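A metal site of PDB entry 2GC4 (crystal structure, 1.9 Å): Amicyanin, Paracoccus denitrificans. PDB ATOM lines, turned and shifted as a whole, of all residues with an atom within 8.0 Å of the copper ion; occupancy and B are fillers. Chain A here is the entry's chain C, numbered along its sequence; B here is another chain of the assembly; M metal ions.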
ATOM      1  N   ILE A  25       5.652  11.648   5.610  1.00  0.00           N
ATOM      2  CA  ILE A  25       6.077  13.008   5.894  1.00  0.00           C
ATOM      3  C   ILE A  25       4.862  13.894   5.707  1.00  0.00           C
ATOM      4  O   ILE A  25       4.277  13.929   4.622  1.00  0.00           O
ATOM      5  CB  ILE A  25       7.182  13.467   4.915  1.00  0.00           C
ATOM      6  CG1 ILE A  25       8.352  12.492   4.944  1.00  0.00           C
ATOM      7  CG2 ILE A  25       7.670  14.854   5.317  1.00  0.00           C
ATOM      8  CD1 ILE A  25       9.458  12.846   3.968  1.00  0.00           C
ATOM      9  N   MET A  28       5.007  19.152   8.229  1.00  0.00           N
ATOM     10  CA  MET A  28       6.374  19.508   8.604  1.00  0.00           C
ATOM     11  C   MET A  28       7.056  18.549   9.570  1.00  0.00           C
ATOM     12  O   MET A  28       7.832  18.973  10.415  1.00  0.00           O
ATOM     13  CB  MET A  28       6.409  20.918   9.214  1.00  0.00           C
ATOM     14  CG  MET A  28       5.832  22.002   8.326  1.00  0.00           C
ATOM     15  SD  MET A  28       6.719  22.141   6.767  1.00  0.00           S
ATOM     16  CE  MET A  28       8.128  23.099   7.263  1.00  0.00           C
ATOM     17  N   LYS A  29       6.776  17.258   9.442  1.00  0.00           N
ATOM     18  CA  LYS A  29       7.411  16.299  10.333  1.00  0.00           C
ATOM     19  C   LYS A  29       7.463  14.878   9.771  1.00  0.00           C
ATOM     20  O   LYS A  29       6.675  14.502   8.914  1.00  0.00           O
ATOM     21  CB  LYS A  29       6.688  16.264  11.688  1.00  0.00           C
ATOM     22  CG  LYS A  29       5.373  15.483  11.674  1.00  0.00           C
ATOM     23  CD  LYS A  29       4.803  15.302  13.084  1.00  0.00           C
ATOM     24  CE  LYS A  29       4.228  16.592  13.626  1.00  0.00           C
ATOM     25  NZ  LYS A  29       3.106  17.088  12.791  1.00  0.00           N
ATOM     26  N   TYR A  30       8.426  14.108  10.262  1.00  0.00           N
ATOM     27  CA  TYR A  30       8.553  12.713   9.888  1.00  0.00           C
ATOM     28  C   TYR A  30       7.631  12.065  10.921  1.00  0.00           C
ATOM     29  O   TYR A  30       7.939  12.073  12.118  1.00  0.00           O
ATOM     30  CB  TYR A  30      10.007  12.252  10.061  1.00  0.00           C
ATOM     31  CG  TYR A  30      10.968  12.973   9.138  1.00  0.00           C
ATOM     32  CD1 TYR A  30      10.894  12.808   7.757  1.00  0.00           C
ATOM     33  CD2 TYR A  30      11.928  13.837   9.650  1.00  0.00           C
ATOM     34  CE1 TYR A  30      11.762  13.492   6.890  1.00  0.00           C
ATOM     35  CE2 TYR A  30      12.806  14.535   8.799  1.00  0.00           C
ATOM     36  CZ  TYR A  30      12.714  14.354   7.420  1.00  0.00           C
ATOM     37  OH  TYR A  30      13.585  15.019   6.585  1.00  0.00           O
ATOM     38  N   ASN A  47       6.325  11.562   0.928  1.00  0.00           N
ATOM     39  CA  ASN A  47       5.832  12.897   1.258  1.00  0.00           C
ATOM     40  C   ASN A  47       4.341  12.899   1.021  1.00  0.00           C
ATOM     41  O   ASN A  47       3.875  12.540  -0.066  1.00  0.00           O
ATOM     42  CB  ASN A  47       6.507  13.960   0.390  1.00  0.00           C
ATOM     43  CG  ASN A  47       6.177  15.377   0.831  1.00  0.00           C
ATOM     44  OD1 ASN A  47       5.522  15.585   1.852  1.00  0.00           O
ATOM     45  ND2 ASN A  47       6.636  16.364   0.060  1.00  0.00           N
ATOM     46  N   GLU A  49       2.391  15.757   1.644  1.00  0.00           N
ATOM     47  CA  GLU A  49       1.896  17.124   1.483  1.00  0.00           C
ATOM     48  C   GLU A  49       2.568  17.873   0.338  1.00  0.00           C
ATOM     49  O   GLU A  49       3.591  17.436  -0.202  1.00  0.00           O
ATOM     50  CB  GLU A  49       2.059  17.904   2.799  1.00  0.00           C
ATOM     51  CG  GLU A  49       3.495  18.161   3.251  1.00  0.00           C
ATOM     52  CD  GLU A  49       3.576  18.854   4.612  1.00  0.00           C
ATOM     53  OE1 GLU A  49       2.543  19.408   5.058  1.00  0.00           O
ATOM     54  OE2 GLU A  49       4.656  18.857   5.227  1.00  0.00           O
ATOM     55  N   MET A  51       4.179  20.745   0.376  1.00  0.00           N
ATOM     56  CA  MET A  51       5.495  21.222   0.771  1.00  0.00           C
ATOM     57  C   MET A  51       6.563  20.163   0.486  1.00  0.00           C
ATOM     58  O   MET A  51       6.505  19.049   1.017  1.00  0.00           O
ATOM     59  CB  MET A  51       5.484  21.535   2.270  1.00  0.00           C
ATOM     60  CG  MET A  51       6.833  21.909   2.846  1.00  0.00           C
ATOM     61  SD  MET A  51       7.311  23.589   2.424  1.00  0.00           S
ATOM     62  CE  MET A  51       6.460  24.497   3.701  1.00  0.00           C
ATOM     63  N   PRO A  52       7.545  20.484  -0.372  1.00  0.00           N
ATOM     64  CA  PRO A  52       8.598  19.522  -0.699  1.00  0.00           C
ATOM     65  C   PRO A  52       9.513  19.212   0.487  1.00  0.00           C
ATOM     66  O   PRO A  52       9.805  20.107   1.288  1.00  0.00           O
ATOM     67  CB  PRO A  52       9.354  20.203  -1.846  1.00  0.00           C
ATOM     68  CG  PRO A  52       8.263  21.037  -2.509  1.00  0.00           C
ATOM     69  CD  PRO A  52       7.573  21.625  -1.307  1.00  0.00           C
ATOM     70  N   HIS A  53       9.945  17.958   0.597  1.00  0.00           N
ATOM     71  CA  HIS A  53      10.830  17.506   1.681  1.00  0.00           C
ATOM     72  C   HIS A  53      11.800  16.452   1.157  1.00  0.00           C
ATOM     73  O   HIS A  53      11.578  15.879   0.083  1.00  0.00           O
ATOM     74  CB  HIS A  53      10.024  16.849   2.819  1.00  0.00           C
ATOM     75  CG  HIS A  53       9.006  17.736   3.452  1.00  0.00           C
ATOM     76  ND1 HIS A  53       9.300  18.802   4.268  1.00  0.00           N
ATOM     77  CD2 HIS A  53       7.650  17.649   3.442  1.00  0.00           C
ATOM     78  CE1 HIS A  53       8.148  19.317   4.724  1.00  0.00           C
ATOM     79  NE2 HIS A  53       7.111  18.652   4.250  1.00  0.00           N
ATOM     80  N   ASN A  54      12.845  16.168   1.920  1.00  0.00           N
ATOM     81  CA  ASN A  54      13.836  15.173   1.551  1.00  0.00           C
ATOM     82  C   ASN A  54      14.452  14.656   2.841  1.00  0.00           C
ATOM     83  O   ASN A  54      14.072  15.085   3.924  1.00  0.00           O
ATOM     84  CB  ASN A  54      14.927  15.791   0.655  1.00  0.00           C
ATOM     85  CG  ASN A  54      15.981  16.557   1.463  1.00  0.00           C
ATOM     86  OD1 ASN A  54      15.689  17.169   2.490  1.00  0.00           O
ATOM     87  ND2 ASN A  54      17.225  16.533   0.977  1.00  0.00           N
ATOM     88  N   VAL A  55      15.407  13.728   2.725  1.00  0.00           N
ATOM     89  CA  VAL A  55      16.099  13.217   3.895  1.00  0.00           C
ATOM     90  C   VAL A  55      17.548  13.572   3.650  1.00  0.00           C
ATOM     91  O   VAL A  55      18.023  13.539   2.509  1.00  0.00           O
ATOM     92  CB  VAL A  55      15.928  11.685   4.070  1.00  0.00           C
ATOM     93  CG1 VAL A  55      14.458  11.367   4.331  1.00  0.00           C
ATOM     94  CG2 VAL A  55      16.429  10.960   2.830  1.00  0.00           C
ATOM     95  N   MET A  71      14.682  15.993  -3.376  1.00  0.00           N
ATOM     96  CA  MET A  71      13.465  16.567  -2.823  1.00  0.00           C
ATOM     97  C   MET A  71      12.249  15.817  -3.372  1.00  0.00           C
ATOM     98  O   MET A  71      12.163  15.544  -4.570  1.00  0.00           O
ATOM     99  CB  MET A  71      13.348  18.055  -3.192  1.00  0.00           C
ATOM    100  CG  MET A  71      14.341  18.953  -2.478  1.00  0.00           C
ATOM    101  SD  MET A  71      14.105  19.021  -0.682  1.00  0.00           S
ATOM    102  CE  MET A  71      12.709  20.120  -0.570  1.00  0.00           C
ATOM    103  N   HIS A  91      17.867  14.807   8.683  1.00  0.00           N
ATOM    104  CA  HIS A  91      17.012  15.985   8.743  1.00  0.00           C
ATOM    105  C   HIS A  91      16.588  16.357   7.328  1.00  0.00           C
ATOM    106  O   HIS A  91      16.966  15.692   6.356  1.00  0.00           O
ATOM    107  CB  HIS A  91      17.737  17.161   9.395  1.00  0.00           C
ATOM    108  CG  HIS A  91      18.849  17.736   8.560  1.00  0.00           C
ATOM    109  ND1 HIS A  91      20.051  17.097   8.389  1.00  0.00           N
ATOM    110  CD2 HIS A  91      18.913  18.871   7.825  1.00  0.00           C
ATOM    111  CE1 HIS A  91      20.821  17.815   7.580  1.00  0.00           C
ATOM    112  NE2 HIS A  91      20.144  18.899   7.228  1.00  0.00           N
ATOM    113  N   CYS A  92      15.806  17.413   7.224  1.00  0.00           N
ATOM    114  CA  CYS A  92      15.337  17.915   5.931  1.00  0.00           C
ATOM    115  C   CYS A  92      16.206  19.126   5.577  1.00  0.00           C
ATOM    116  O   CYS A  92      16.255  20.106   6.312  1.00  0.00           O
ATOM    117  CB  CYS A  92      13.871  18.317   6.055  1.00  0.00           C
ATOM    118  SG  CYS A  92      13.137  18.746   4.488  1.00  0.00           S
ATOM    119  N   THR A  93      16.884  19.044   4.433  1.00  0.00           N
ATOM    120  CA  THR A  93      17.792  20.105   3.986  1.00  0.00           C
ATOM    121  C   THR A  93      17.308  21.541   4.196  1.00  0.00           C
ATOM    122  O   THR A  93      17.925  22.296   4.931  1.00  0.00           O
ATOM    123  CB  THR A  93      18.187  19.888   2.510  1.00  0.00           C
ATOM    124  OG1 THR A  93      18.864  18.627   2.399  1.00  0.00           O
ATOM    125  CG2 THR A  93      19.125  20.998   2.036  1.00  0.00           C
ATOM    126  N   PRO A  94      16.185  21.944   3.561  1.00  0.00           N
ATOM    127  CA  PRO A  94      15.701  23.315   3.744  1.00  0.00           C
ATOM    128  C   PRO A  94      15.023  23.589   5.089  1.00  0.00           C
ATOM    129  O   PRO A  94      14.779  24.744   5.447  1.00  0.00           O
ATOM    130  CB  PRO A  94      14.723  23.489   2.575  1.00  0.00           C
ATOM    131  CG  PRO A  94      14.143  22.110   2.440  1.00  0.00           C
ATOM    132  CD  PRO A  94      15.365  21.222   2.564  1.00  0.00           C
ATOM    133  N   HIS A  95      14.732  22.528   5.829  1.00  0.00           N
ATOM    134  CA  HIS A  95      14.055  22.641   7.118  1.00  0.00           C
ATOM    135  C   HIS A  95      14.838  21.912   8.212  1.00  0.00           C
ATOM    136  O   HIS A  95      14.415  20.855   8.686  1.00  0.00           O
ATOM    137  CB  HIS A  95      12.647  22.044   6.990  1.00  0.00           C
ATOM    138  CG  HIS A  95      11.910  22.494   5.762  1.00  0.00           C
ATOM    139  ND1 HIS A  95      11.013  21.713   5.076  1.00  0.00           N
ATOM    140  CD2 HIS A  95      11.944  23.676   5.106  1.00  0.00           C
ATOM    141  CE1 HIS A  95      10.550  22.423   4.033  1.00  0.00           C
ATOM    142  NE2 HIS A  95      11.087  23.620   4.003  1.00  0.00           N
ATOM    143  N   PRO A  96      15.986  22.474   8.628  1.00  0.00           N
ATOM    144  CA  PRO A  96      16.852  21.885   9.661  1.00  0.00           C
ATOM    145  C   PRO A  96      16.145  21.449  10.936  1.00  0.00           C
ATOM    146  O   PRO A  96      16.615  20.551  11.639  1.00  0.00           O
ATOM    147  CB  PRO A  96      17.878  22.997   9.915  1.00  0.00           C
ATOM    148  CG  PRO A  96      17.984  23.664   8.580  1.00  0.00           C
ATOM    149  CD  PRO A  96      16.532  23.762   8.161  1.00  0.00           C
ATOM    150  N   PHE A  97      15.014  22.068  11.246  1.00  0.00           N
ATOM    151  CA  PHE A  97      14.255  21.725  12.440  1.00  0.00           C
ATOM    152  C   PHE A  97      13.531  20.383  12.311  1.00  0.00           C
ATOM    153  O   PHE A  97      13.065  19.830  13.311  1.00  0.00           O
ATOM    154  CB  PHE A  97      13.236  22.824  12.761  1.00  0.00           C
ATOM    155  CG  PHE A  97      12.366  23.203  11.601  1.00  0.00           C
ATOM    156  CD1 PHE A  97      12.839  24.055  10.606  1.00  0.00           C
ATOM    157  CD2 PHE A  97      11.083  22.669  11.478  1.00  0.00           C
ATOM    158  CE1 PHE A  97      12.032  24.395   9.514  1.00  0.00           C
ATOM    159  CE2 PHE A  97      10.279  23.001  10.386  1.00  0.00           C
ATOM    160  CZ  PHE A  97      10.753  23.864   9.404  1.00  0.00           C
ATOM    161  N   MET A  98      13.412  19.887  11.081  1.00  0.00           N
ATOM    162  CA  MET A  98      12.757  18.592  10.843  1.00  0.00           C
ATOM    163  C   MET A  98      13.791  17.509  11.023  1.00  0.00           C
ATOM    164  O   MET A  98      14.716  17.402  10.215  1.00  0.00           O
ATOM    165  CB  MET A  98      12.222  18.505   9.420  1.00  0.00           C
ATOM    166  CG  MET A  98      10.860  19.100   9.222  1.00  0.00           C
ATOM    167  SD  MET A  98      10.345  18.908   7.514  1.00  0.00           S
ATOM    168  CE  MET A  98       9.868  17.166   7.461  1.00  0.00           C
ATOM    169  N   ARG A  99      13.652  16.696  12.068  1.00  0.00           N
ATOM    170  CA  ARG A  99      14.613  15.647  12.328  1.00  0.00           C
ATOM    171  C   ARG A  99      13.967  14.277  12.526  1.00  0.00           C
ATOM    172  O   ARG A  99      12.843  14.160  13.010  1.00  0.00           O
ATOM    173  CB  ARG A  99      15.467  15.993  13.540  1.00  0.00           C
ATOM    174  CG  ARG A  99      16.274  17.281  13.384  1.00  0.00           C
ATOM    175  CD  ARG A  99      17.213  17.505  14.557  1.00  0.00           C
ATOM    176  NE  ARG A  99      17.970  18.747  14.419  1.00  0.00           N
ATOM    177  CZ  ARG A  99      17.466  19.963  14.591  1.00  0.00           C
ATOM    178  NH1 ARG A  99      18.234  21.038  14.434  1.00  0.00           N
ATOM    179  NH2 ARG A  99      16.191  20.114  14.921  1.00  0.00           N
ATOM    180  N   GLU B 101      11.154  27.959   5.903  1.00  0.00           N
ATOM    181  CA  GLU B 101      10.361  27.337   4.849  1.00  0.00           C
ATOM    182  C   GLU B 101       9.654  28.390   3.989  1.00  0.00           C
ATOM    183  O   GLU B 101       9.354  28.144   2.831  1.00  0.00           O
ATOM    184  CB  GLU B 101       9.338  26.364   5.450  1.00  0.00           C
ATOM    185  CG  GLU B 101       8.312  27.004   6.388  1.00  0.00           C
ATOM    186  CD  GLU B 101       8.702  26.920   7.854  1.00  0.00           C
ATOM    187  OE1 GLU B 101       9.900  27.048   8.170  1.00  0.00           O
ATOM    188  OE2 GLU B 101       7.799  26.729   8.691  1.00  0.00           O
HETATM  189 CU    CU M   1      11.121  19.549   5.136  1.00  0.00          CU
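ND1 of His 53 binds the copper ion, at 2.2 Å.
ND1 of His 95 binds the copper ion (2.2 Å).
The copper ion is bound by the side-chain sulfur (SG) of Cys 92, at 2.3 Å.
SD of Met 98 is bound to the copper ion, at 2.6 Å.
The copper ion has four donor atoms within binding distance.
OH of Tyr 30 lies within hydrogen-bond range of N of Cys 92, at 3.3 Å.
O of Met 51 sits close to NE2 of His 53, 3.3 Å away.
SG of Cys 92 lies close to OD1 of Asn 54 (3.6 Å).
A ring nitrogen (NE2) of His 53 is in hydrogen-bond range of the side-chain carboxylate (OE2) of Glu 49, 2.7 Å away.
Within 4 Å of the copper ion: His 53, Cys 92, His 95 and Met 98.
The nearest printed residue that does not touch the copper ion is Pro 52 (4.1 Å).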
